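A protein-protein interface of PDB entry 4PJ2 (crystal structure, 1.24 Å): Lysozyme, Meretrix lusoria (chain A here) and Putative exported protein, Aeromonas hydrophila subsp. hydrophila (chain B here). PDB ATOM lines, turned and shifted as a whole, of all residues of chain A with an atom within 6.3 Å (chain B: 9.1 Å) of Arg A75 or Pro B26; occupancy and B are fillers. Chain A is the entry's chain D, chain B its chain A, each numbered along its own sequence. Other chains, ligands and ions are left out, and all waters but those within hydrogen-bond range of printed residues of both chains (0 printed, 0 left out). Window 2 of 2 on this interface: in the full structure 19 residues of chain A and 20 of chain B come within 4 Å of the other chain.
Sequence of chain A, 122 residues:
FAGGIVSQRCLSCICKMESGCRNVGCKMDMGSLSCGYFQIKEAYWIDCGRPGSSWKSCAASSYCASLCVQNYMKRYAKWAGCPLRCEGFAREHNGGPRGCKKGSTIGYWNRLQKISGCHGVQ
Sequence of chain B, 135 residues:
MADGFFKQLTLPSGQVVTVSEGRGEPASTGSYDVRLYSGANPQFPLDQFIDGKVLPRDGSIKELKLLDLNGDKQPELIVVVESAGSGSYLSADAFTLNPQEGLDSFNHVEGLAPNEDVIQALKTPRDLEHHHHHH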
ATOM      1  N   ILE A   5      39.246 -37.204 -22.113  1.00  0.00           N
ATOM      2  CA  ILE A   5      40.182 -36.222 -21.575  1.00  0.00           C
ATOM      3  C   ILE A   5      40.610 -36.486 -20.139  1.00  0.00           C
ATOM      4  O   ILE A   5      41.610 -35.943 -19.684  1.00  0.00           O
ATOM      5  CB  ILE A   5      39.648 -34.788 -21.686  1.00  0.00           C
ATOM      6  CG1 ILE A   5      38.403 -34.571 -20.831  1.00  0.00           C
ATOM      7  CG2 ILE A   5      39.384 -34.467 -23.162  1.00  0.00           C
ATOM      8  CD1 ILE A   5      37.932 -33.134 -20.866  1.00  0.00           C
ATOM      9  N   ILE A  46      21.829 -36.802 -18.213  1.00  0.00           N
ATOM     10  CA  ILE A  46      21.218 -36.070 -19.314  1.00  0.00           C
ATOM     11  C   ILE A  46      22.274 -35.200 -20.007  1.00  0.00           C
ATOM     12  O   ILE A  46      22.412 -35.223 -21.229  1.00  0.00           O
ATOM     13  CB  ILE A  46      20.024 -35.202 -18.827  1.00  0.00           C
ATOM     14  CG1 ILE A  46      18.849 -36.110 -18.444  1.00  0.00           C
ATOM     15  CG2 ILE A  46      19.613 -34.173 -19.882  1.00  0.00           C
ATOM     16  CD1 ILE A  46      17.720 -35.406 -17.700  1.00  0.00           C
ATOM     17  N   ASP A  47      23.062 -34.475 -19.225  1.00  0.00           N
ATOM     18  CA  ASP A  47      24.026 -33.544 -19.795  1.00  0.00           C
ATOM     19  C   ASP A  47      25.254 -34.246 -20.386  1.00  0.00           C
ATOM     20  O   ASP A  47      25.923 -33.669 -21.243  1.00  0.00           O
ATOM     21  CB  ASP A  47      24.491 -32.550 -18.744  1.00  0.00           C
ATOM     22  CG  ASP A  47      23.464 -31.486 -18.438  1.00  0.00           C
ATOM     23  OD1 ASP A  47      22.377 -31.436 -19.063  1.00  0.00           O
ATOM     24  OD2 ASP A  47      23.774 -30.656 -17.559  1.00  0.00           O
ATOM     25  N   CYS A  48      25.552 -35.467 -19.955  1.00  0.00           N
ATOM     26  CA  CYS A  48      26.706 -36.182 -20.501  1.00  0.00           C
ATOM     27  C   CYS A  48      26.337 -36.924 -21.783  1.00  0.00           C
ATOM     28  O   CYS A  48      27.099 -37.754 -22.267  1.00  0.00           O
ATOM     29  CB  CYS A  48      27.303 -37.148 -19.473  1.00  0.00           C
ATOM     30  SG  CYS A  48      26.393 -38.676 -19.244  1.00  0.00           S
ATOM     31  N   GLY A  49      25.162 -36.619 -22.325  1.00  0.00           N
ATOM     32  CA  GLY A  49      24.764 -37.105 -23.634  1.00  0.00           C
ATOM     33  C   GLY A  49      23.918 -38.364 -23.629  1.00  0.00           C
ATOM     34  O   GLY A  49      23.726 -38.995 -24.661  1.00  0.00           O
ATOM     35  N   GLN A  70      33.527 -38.898 -18.751  1.00  0.00           N
ATOM     36  CA  GLN A  70      34.342 -38.348 -19.833  1.00  0.00           C
ATOM     37  C   GLN A  70      33.577 -37.296 -20.643  1.00  0.00           C
ATOM     38  O   GLN A  70      34.115 -36.223 -20.949  1.00  0.00           O
ATOM     39  CB  GLN A  70      34.833 -39.458 -20.768  1.00  0.00           C
ATOM     40  CG  GLN A  70      35.838 -40.413 -20.150  1.00  0.00           C
ATOM     41  CD  GLN A  70      37.234 -39.827 -20.021  1.00  0.00           C
ATOM     42  OE1 GLN A  70      37.429 -38.619 -20.086  1.00  0.00           O
ATOM     43  NE2 GLN A  70      38.216 -40.697 -19.844  1.00  0.00           N
ATOM     44  N   ASN A  71      32.339 -37.607 -21.015  1.00  0.00           N
ATOM     45  CA  ASN A  71      31.513 -36.678 -21.786  1.00  0.00           C
ATOM     46  C   ASN A  71      31.167 -35.428 -20.989  1.00  0.00           C
ATOM     47  O   ASN A  71      31.131 -34.344 -21.547  1.00  0.00           O
ATOM     48  CB  ASN A  71      30.205 -37.313 -22.249  1.00  0.00           C
ATOM     49  CG  ASN A  71      30.395 -38.370 -23.303  1.00  0.00           C
ATOM     50  OD1 ASN A  71      31.463 -38.498 -23.893  1.00  0.00           O
ATOM     51  ND2 ASN A  71      29.341 -39.117 -23.572  1.00  0.00           N
ATOM     52  N   TYR A  72      30.887 -35.577 -19.696  1.00  0.00           N
ATOM     53  CA  TYR A  72      30.593 -34.449 -18.828  1.00  0.00           C
ATOM     54  C   TYR A  72      31.773 -33.484 -18.753  1.00  0.00           C
ATOM     55  O   TYR A  72      31.604 -32.266 -18.867  1.00  0.00           O
ATOM     56  CB  TYR A  72      30.244 -34.955 -17.439  1.00  0.00           C
ATOM     57  CG  TYR A  72      29.480 -33.968 -16.588  1.00  0.00           C
ATOM     58  CD1 TYR A  72      30.123 -33.149 -15.669  1.00  0.00           C
ATOM     59  CD2 TYR A  72      28.096 -33.884 -16.672  1.00  0.00           C
ATOM     60  CE1 TYR A  72      29.405 -32.268 -14.862  1.00  0.00           C
ATOM     61  CE2 TYR A  72      27.378 -32.997 -15.876  1.00  0.00           C
ATOM     62  CZ  TYR A  72      28.032 -32.190 -14.977  1.00  0.00           C
ATOM     63  OH  TYR A  72      27.303 -31.332 -14.170  1.00  0.00           O
ATOM     64  N   MET A  73      32.980 -34.028 -18.592  1.00  0.00           N
ATOM     65  CA  MET A  73      34.156 -33.191 -18.515  1.00  0.00           C
ATOM     66  C   MET A  73      34.443 -32.531 -19.865  1.00  0.00           C
ATOM     67  O   MET A  73      34.822 -31.379 -19.898  1.00  0.00           O
ATOM     68  CB  MET A  73      35.375 -33.994 -18.005  1.00  0.00           C
ATOM     69  CG  MET A  73      35.191 -34.600 -16.606  1.00  0.00           C
ATOM     70  SD  MET A  73      34.531 -33.409 -15.437  1.00  0.00           S
ATOM     71  CE  MET A  73      33.708 -34.536 -14.309  1.00  0.00           C
ATOM     72  N   LYS A  74      34.261 -33.267 -20.958  1.00  0.00           N
ATOM     73  CA  LYS A  74      34.420 -32.696 -22.300  1.00  0.00           C
ATOM     74  C   LYS A  74      33.473 -31.517 -22.510  1.00  0.00           C
ATOM     75  O   LYS A  74      33.847 -30.505 -23.099  1.00  0.00           O
ATOM     76  CB  LYS A  74      34.168 -33.772 -23.351  1.00  0.00           C
ATOM     77  CG  LYS A  74      34.331 -33.320 -24.788  1.00  0.00           C
ATOM     78  CD  LYS A  74      34.247 -34.507 -25.745  1.00  0.00           C
ATOM     79  CE  LYS A  74      34.135 -34.073 -27.205  1.00  0.00           C
ATOM     80  NZ  LYS A  74      33.992 -35.240 -28.125  1.00  0.00           N
ATOM     81  N   ARG A  75      32.250 -31.649 -22.019  1.00  0.00           N
ATOM     82  CA  ARG A  75      31.264 -30.593 -22.162  1.00  0.00           C
ATOM     83  C   ARG A  75      31.586 -29.368 -21.308  1.00  0.00           C
ATOM     84  O   ARG A  75      31.483 -28.230 -21.798  1.00  0.00           O
ATOM     85  CB  ARG A  75      29.875 -31.120 -21.810  1.00  0.00           C
ATOM     86  CG  ARG A  75      28.790 -30.060 -21.862  1.00  0.00           C
ATOM     87  CD  ARG A  75      27.418 -30.677 -21.766  1.00  0.00           C
ATOM     88  NE  ARG A  75      26.401 -29.660 -22.002  1.00  0.00           N
ATOM     89  CZ  ARG A  75      25.149 -29.924 -22.347  1.00  0.00           C
ATOM     90  NH1 ARG A  75      24.746 -31.185 -22.440  1.00  0.00           N
ATOM     91  NH2 ARG A  75      24.301 -28.930 -22.595  1.00  0.00           N
ATOM     92  N   TYR A  76      31.979 -29.583 -20.047  1.00  0.00           N
ATOM     93  CA  TYR A  76      31.997 -28.493 -19.076  1.00  0.00           C
ATOM     94  C   TYR A  76      33.362 -28.001 -18.601  1.00  0.00           C
ATOM     95  O   TYR A  76      33.504 -26.834 -18.256  1.00  0.00           O
ATOM     96  CB  TYR A  76      31.171 -28.871 -17.856  1.00  0.00           C
ATOM     97  CG  TYR A  76      29.689 -28.898 -18.076  1.00  0.00           C
ATOM     98  CD1 TYR A  76      29.019 -27.768 -18.512  1.00  0.00           C
ATOM     99  CD2 TYR A  76      28.952 -30.045 -17.807  1.00  0.00           C
ATOM    100  CE1 TYR A  76      27.652 -27.774 -18.652  1.00  0.00           C
ATOM    101  CE2 TYR A  76      27.575 -30.049 -17.957  1.00  0.00           C
ATOM    102  CZ  TYR A  76      26.940 -28.907 -18.386  1.00  0.00           C
ATOM    103  OH  TYR A  76      25.570 -28.814 -18.534  1.00  0.00           O
ATOM    104  N   ALA A  77      34.348 -28.887 -18.482  1.00  0.00           N
ATOM    105  CA  ALA A  77      35.517 -28.547 -17.685  1.00  0.00           C
ATOM    106  C   ALA A  77      36.326 -27.379 -18.268  1.00  0.00           C
ATOM    107  O   ALA A  77      36.645 -26.423 -17.578  1.00  0.00           O
ATOM    108  CB  ALA A  77      36.398 -29.773 -17.504  1.00  0.00           C
ATOM    109  N   LYS A  78      36.665 -27.458 -19.544  1.00  0.00           N
ATOM    110  CA  LYS A  78      37.462 -26.404 -20.154  1.00  0.00           C
ATOM    111  C   LYS A  78      36.793 -25.049 -19.992  1.00  0.00           C
ATOM    112  O   LYS A  78      37.420 -24.067 -19.611  1.00  0.00           O
ATOM    113  CB  LYS A  78      37.664 -26.683 -21.638  1.00  0.00           C
ATOM    114  CG  LYS A  78      38.446 -25.600 -22.331  1.00  0.00           C
ATOM    115  CD  LYS A  78      38.723 -25.964 -23.789  1.00  0.00           C
ATOM    116  CE  LYS A  78      39.647 -24.975 -24.478  1.00  0.00           C
ATOM    117  NZ  LYS A  78      41.037 -25.059 -23.915  1.00  0.00           N
ATOM    118  N   TRP A  79      35.502 -25.022 -20.277  1.00  0.00           N
ATOM    119  CA  TRP A  79      34.765 -23.770 -20.414  1.00  0.00           C
ATOM    120  C   TRP A  79      34.481 -23.119 -19.068  1.00  0.00           C
ATOM    121  O   TRP A  79      34.184 -21.931 -18.994  1.00  0.00           O
ATOM    122  CB  TRP A  79      33.485 -24.030 -21.213  1.00  0.00           C
ATOM    123  CG  TRP A  79      33.837 -24.771 -22.473  1.00  0.00           C
ATOM    124  CD1 TRP A  79      33.562 -26.066 -22.774  1.00  0.00           C
ATOM    125  CD2 TRP A  79      34.583 -24.259 -23.567  1.00  0.00           C
ATOM    126  NE1 TRP A  79      34.092 -26.397 -23.993  1.00  0.00           N
ATOM    127  CE2 TRP A  79      34.719 -25.297 -24.506  1.00  0.00           C
ATOM    128  CE3 TRP A  79      35.155 -23.020 -23.846  1.00  0.00           C
ATOM    129  CZ2 TRP A  79      35.401 -25.129 -25.708  1.00  0.00           C
ATOM    130  CZ3 TRP A  79      35.840 -22.865 -25.023  1.00  0.00           C
ATOM    131  CH2 TRP A  79      35.954 -23.909 -25.941  1.00  0.00           C
ATOM    132  N   GLY B   4      11.585 -28.926 -18.515  1.00  0.00           N
ATOM    133  CA  GLY B   4      12.053 -27.800 -17.727  1.00  0.00           C
ATOM    134  C   GLY B   4      11.083 -27.420 -16.616  1.00  0.00           C
ATOM    135  O   GLY B   4       9.870 -27.387 -16.816  1.00  0.00           O
ATOM    136  N   PHE B   5      11.628 -27.133 -15.440  1.00  0.00           N
ATOM    137  CA  PHE B   5      10.830 -26.825 -14.263  1.00  0.00           C
ATOM    138  C   PHE B   5       9.909 -25.645 -14.508  1.00  0.00           C
ATOM    139  O   PHE B   5      10.339 -24.638 -15.043  1.00  0.00           O
ATOM    140  CB  PHE B   5      11.773 -26.493 -13.116  1.00  0.00           C
ATOM    141  CG  PHE B   5      11.090 -26.262 -11.813  1.00  0.00           C
ATOM    142  CD1 PHE B   5      11.002 -27.276 -10.872  1.00  0.00           C
ATOM    143  CD2 PHE B   5      10.551 -25.025 -11.517  1.00  0.00           C
ATOM    144  CE1 PHE B   5      10.377 -27.058  -9.672  1.00  0.00           C
ATOM    145  CE2 PHE B   5       9.922 -24.802 -10.319  1.00  0.00           C
ATOM    146  CZ  PHE B   5       9.836 -25.822  -9.393  1.00  0.00           C
ATOM    147  N   GLU B  21      12.760 -22.754 -15.112  1.00  0.00           N
ATOM    148  CA  GLU B  21      14.131 -22.847 -15.615  1.00  0.00           C
ATOM    149  C   GLU B  21      14.210 -22.299 -17.031  1.00  0.00           C
ATOM    150  O   GLU B  21      13.251 -22.339 -17.788  1.00  0.00           O
ATOM    151  CB  GLU B  21      14.605 -24.301 -15.560  1.00  0.00           C
ATOM    152  CG  GLU B  21      14.943 -24.721 -14.124  1.00  0.00           C
ATOM    153  CD  GLU B  21      15.312 -26.180 -13.967  1.00  0.00           C
ATOM    154  OE1 GLU B  21      15.060 -26.960 -14.900  1.00  0.00           O
ATOM    155  OE2 GLU B  21      15.848 -26.560 -12.899  1.00  0.00           O
ATOM    156  N   GLY B  22      15.367 -21.787 -17.401  1.00  0.00           N
ATOM    157  CA  GLY B  22      15.541 -21.263 -18.749  1.00  0.00           C
ATOM    158  C   GLY B  22      15.383 -22.313 -19.840  1.00  0.00           C
ATOM    159  O   GLY B  22      15.851 -23.441 -19.716  1.00  0.00           O
ATOM    160  N   ARG B  23      14.714 -21.932 -20.922  1.00  0.00           N
ATOM    161  CA  ARG B  23      14.432 -22.860 -22.004  1.00  0.00           C
ATOM    162  C   ARG B  23      15.691 -23.177 -22.800  1.00  0.00           C
ATOM    163  O   ARG B  23      16.507 -22.298 -23.083  1.00  0.00           O
ATOM    164  CB  ARG B  23      13.340 -22.308 -22.922  1.00  0.00           C
ATOM    165  CG  ARG B  23      13.055 -23.177 -24.133  1.00  0.00           C
ATOM    166  CD  ARG B  23      11.731 -22.809 -24.768  1.00  0.00           C
ATOM    167  NE  ARG B  23      11.527 -23.562 -25.997  1.00  0.00           N
ATOM    168  CZ  ARG B  23      10.426 -23.514 -26.735  1.00  0.00           C
ATOM    169  NH1 ARG B  23       9.418 -22.738 -26.374  1.00  0.00           N
ATOM    170  NH2 ARG B  23      10.345 -24.238 -27.841  1.00  0.00           N
ATOM    171  N   GLY B  24      15.839 -24.455 -23.148  1.00  0.00           N
ATOM    172  CA  GLY B  24      16.948 -24.917 -23.963  1.00  0.00           C
ATOM    173  C   GLY B  24      18.247 -25.136 -23.212  1.00  0.00           C
ATOM    174  O   GLY B  24      19.237 -25.539 -23.785  1.00  0.00           O
ATOM    175  N   GLU B  25      18.246 -24.860 -21.919  1.00  0.00           N
ATOM    176  CA  GLU B  25      19.440 -24.958 -21.096  1.00  0.00           C
ATOM    177  C   GLU B  25      19.725 -26.391 -20.679  1.00  0.00           C
ATOM    178  O   GLU B  25      18.824 -27.252 -20.663  1.00  0.00           O
ATOM    179  CB  GLU B  25      19.271 -24.088 -19.848  1.00  0.00           C
ATOM    180  CG  GLU B  25      19.223 -22.609 -20.151  1.00  0.00           C
ATOM    181  CD  GLU B  25      18.998 -21.767 -18.908  1.00  0.00           C
ATOM    182  OE1 GLU B  25      18.722 -22.349 -17.821  1.00  0.00           O
ATOM    183  OE2 GLU B  25      19.107 -20.533 -19.017  1.00  0.00           O
ATOM    184  N   PRO B  26      20.973 -26.644 -20.267  1.00  0.00           N
ATOM    185  CA  PRO B  26      21.259 -27.968 -19.717  1.00  0.00           C
ATOM    186  C   PRO B  26      20.609 -28.203 -18.365  1.00  0.00           C
ATOM    187  O   PRO B  26      20.138 -27.284 -17.696  1.00  0.00           O
ATOM    188  CB  PRO B  26      22.776 -27.959 -19.549  1.00  0.00           C
ATOM    189  CG  PRO B  26      23.190 -26.559 -19.564  1.00  0.00           C
ATOM    190  CD  PRO B  26      22.166 -25.784 -20.305  1.00  0.00           C
ATOM    191  N   ALA B  27      20.598 -29.463 -17.968  1.00  0.00           N
ATOM    192  CA  ALA B  27      20.057 -29.814 -16.675  1.00  0.00           C
ATOM    193  C   ALA B  27      20.892 -29.281 -15.512  1.00  0.00           C
ATOM    194  O   ALA B  27      20.344 -28.910 -14.487  1.00  0.00           O
ATOM    195  CB  ALA B  27      19.896 -31.314 -16.569  1.00  0.00           C
ATOM    196  N   SER B  28      22.211 -29.252 -15.677  1.00  0.00           N
ATOM    197  CA  SER B  28      23.114 -29.018 -14.551  1.00  0.00           C
ATOM    198  C   SER B  28      23.346 -27.570 -14.230  1.00  0.00           C
ATOM    199  O   SER B  28      23.880 -27.262 -13.163  1.00  0.00           O
ATOM    200  CB  SER B  28      24.502 -29.610 -14.812  1.00  0.00           C
ATOM    201  OG  SER B  28      24.492 -30.996 -15.040  1.00  0.00           O
ATOM    202  N   THR B  29      23.058 -26.661 -15.162  1.00  0.00           N
ATOM    203  CA  THR B  29      23.428 -25.270 -14.967  1.00  0.00           C
ATOM    204  C   THR B  29      22.609 -24.405 -15.894  1.00  0.00           C
ATOM    205  O   THR B  29      22.094 -24.894 -16.888  1.00  0.00           O
ATOM    206  CB  THR B  29      24.964 -25.068 -15.205  1.00  0.00           C
ATOM    207  OG1 THR B  29      25.361 -23.744 -14.866  1.00  0.00           O
ATOM    208  CG2 THR B  29      25.387 -25.359 -16.649  1.00  0.00           C
ATOM    209  N   GLY B  30      22.513 -23.120 -15.583  1.00  0.00           N
ATOM    210  CA  GLY B  30      21.806 -22.187 -16.443  1.00  0.00           C
ATOM    211  C   GLY B  30      21.194 -21.105 -15.595  1.00  0.00           C
ATOM    212  O   GLY B  30      21.875 -20.472 -14.793  1.00  0.00           O
ATOM    213  N   SER B  31      19.899 -20.893 -15.772  1.00  0.00           N
ATOM    214  CA  SER B  31      19.188 -19.819 -15.108  1.00  0.00           C
ATOM    215  C   SER B  31      17.814 -20.297 -14.699  1.00  0.00           C
ATOM    216  O   SER B  31      17.325 -21.327 -15.136  1.00  0.00           O
ATOM    217  CB  SER B  31      19.055 -18.614 -16.036  1.00  0.00           C
ATOM    218  OG  SER B  31      18.175 -18.915 -17.116  1.00  0.00           O
ATOM    219  N   ARG B  57      21.400 -20.503 -11.940  1.00  0.00           N
ATOM    220  CA  ARG B  57      21.195 -21.698 -11.136  1.00  0.00           C
ATOM    221  C   ARG B  57      22.321 -22.653 -11.302  1.00  0.00           C
ATOM    222  O   ARG B  57      22.711 -23.035 -12.397  1.00  0.00           O
ATOM    223  CB  ARG B  57      19.892 -22.422 -11.407  1.00  0.00           C
ATOM    224  CG  ARG B  57      19.718 -22.812 -12.811  1.00  0.00           C
ATOM    225  CD  ARG B  57      18.484 -23.719 -13.101  1.00  0.00           C
ATOM    226  NE  ARG B  57      18.446 -23.894 -14.545  1.00  0.00           N
ATOM    227  CZ  ARG B  57      18.932 -24.918 -15.225  1.00  0.00           C
ATOM    228  NH1 ARG B  57      19.440 -25.973 -14.617  1.00  0.00           N
ATOM    229  NH2 ARG B  57      18.873 -24.903 -16.546  1.00  0.00           N
ATOM    230  N   ASP B  58      22.834 -23.057 -10.155  1.00  0.00           N
ATOM    231  CA  ASP B  58      23.895 -24.038 -10.103  1.00  0.00           C
ATOM    232  C   ASP B  58      23.289 -25.382  -9.765  1.00  0.00           C
ATOM    233  O   ASP B  58      23.390 -25.884  -8.622  1.00  0.00           O
ATOM    234  CB  ASP B  58      24.949 -23.653  -9.095  1.00  0.00           C
ATOM    235  CG  ASP B  58      26.055 -24.652  -9.048  1.00  0.00           C
ATOM    236  OD1 ASP B  58      26.219 -25.409 -10.035  1.00  0.00           O
ATOM    237  OD2 ASP B  58      26.756 -24.692  -8.029  1.00  0.00           O
ATOM    238  N   GLY B  59      22.630 -25.953 -10.751  1.00  0.00           N
ATOM    239  CA  GLY B  59      21.988 -27.236 -10.637  1.00  0.00           C
ATOM    240  C   GLY B  59      20.568 -27.121 -11.098  1.00  0.00           C
ATOM    241  O   GLY B  59      20.234 -26.248 -11.896  1.00  0.00           O
ATOM    242  N   SER B  60      19.734 -28.008 -10.595  1.00  0.00           N
ATOM    243  CA  SER B  60      18.317 -28.073 -10.927  1.00  0.00           C
ATOM    244  C   SER B  60      17.467 -27.561  -9.766  1.00  0.00           C
ATOM    245  O   SER B  60      17.800 -27.783  -8.596  1.00  0.00           O
ATOM    246  CB  SER B  60      17.924 -29.525 -11.191  1.00  0.00           C
ATOM    247  OG  SER B  60      18.863 -30.169 -12.021  1.00  0.00           O
ATOM    248  N   ILE B  61      16.356 -26.912 -10.070  1.00  0.00           N
ATOM    249  CA  ILE B  61      15.469 -26.473  -9.013  1.00  0.00           C
ATOM    250  C   ILE B  61      14.880 -27.701  -8.358  1.00  0.00           C
ATOM    251  O   ILE B  61      14.340 -28.588  -9.031  1.00  0.00           O
ATOM    252  CB  ILE B  61      14.361 -25.592  -9.556  1.00  0.00           C
ATOM    253  CG1 ILE B  61      14.953 -24.294 -10.124  1.00  0.00           C
ATOM    254  CG2 ILE B  61      13.347 -25.291  -8.463  1.00  0.00           C
ATOM    255  CD1 ILE B  61      13.933 -23.322 -10.678  1.00  0.00           C
ATOM    256  N   ALA B  84      24.240 -30.602  -9.650  1.00  0.00           N
ATOM    257  CA  ALA B  84      24.240 -31.825 -10.441  1.00  0.00           C
ATOM    258  C   ALA B  84      25.413 -32.734 -10.118  1.00  0.00           C
ATOM    259  O   ALA B  84      25.407 -33.870 -10.549  1.00  0.00           O
ATOM    260  CB  ALA B  84      24.263 -31.502 -11.935  1.00  0.00           C
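Among the printed residues, merely in contact across the chains: Tyr A76 with Pro B26 (3.1 Å), Asp A47 with Pro B26 (3.5 Å), Arg A75 with Pro B26 (3.5 Å), Tyr A72 with Ala B84 (3.8 Å), Tyr A76 with Thr B29 (3.9 Å) and Tyr A76 with Ser B28 (3.95 Å).
Of chain B, only Pro B26 (3.5 Å), Ala B27 (2.9 Å) and Ser B28 (2.6 Å) come within 4 Å of Asp A47.
Printed residues of chain B within 4 Å of Tyr A72: Ser B28 and Ala B84.
Printed residues of chain B within 4 Å of Arg A75: Pro B26.
Of chain A, only Asp A47, Arg A75 and Tyr A76 come within 4 Å of Pro B26.
Printed residues of chain A within 4 Å of Ala B27: Asp A47.
Printed residues of chain A within 4 Å of Thr B29: Tyr A76.
The nearest residue of chain B that does not touch Arg A75 is Glu B25 (5.6 Å).
The nearest residue of chain A that does not touch Pro B26 is Ile A46 (6.2 Å).
The backbone NH of Ala B27 sits at hydrogen-bond distance from the side-chain carboxylate of Asp A47, at 2.9 Å.
The side-chain hydroxyl (OG) of Ser B28 is in hydrogen-bond range of the side-chain carboxylate (OD2) of Asp A47, at 2.6 Å.
The side-chain hydroxyl (OG) of Ser B28 is in hydrogen-bond range of the side-chain hydroxyl (OH) of Tyr A72.
O of Pro B26 sits at hydrogen-bond distance from NH2 of Arg B57 (2.9 Å).
The backbone carbonyl oxygen (O) of Ala B27 sits at hydrogen-bond distance from the guanidinium group (NH1) of Arg B57, 3.1 Å away.
The backbone carbonyl oxygen of Ala B27 is in hydrogen-bond range of the side-chain hydroxyl of Ser B60 (3.1 Å).
O of Ser B28 is in hydrogen-bond range of N of Gly B59.
The backbone carbonyl oxygen (O) of Asp A47 is in hydrogen-bond range of the guanidinium group (NH1) of Arg A75.
The side-chain hydroxyl of Tyr A76 lies within hydrogen-bond range of the side-chain carboxylate of Asp A47.
Along chain A the printed residues that touch a printed residue of chain B span positions 47 to 76.
Printed residues of chain B that touch a printed residue of chain A: Pro B26, Ala B27, Ser B28, Thr B29 and Ala B84.
Hydrophobic or aromatic side chains of chain B within 4 Å of the printed part of chain A: Pro B26, Ala B27 and Ala B84.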
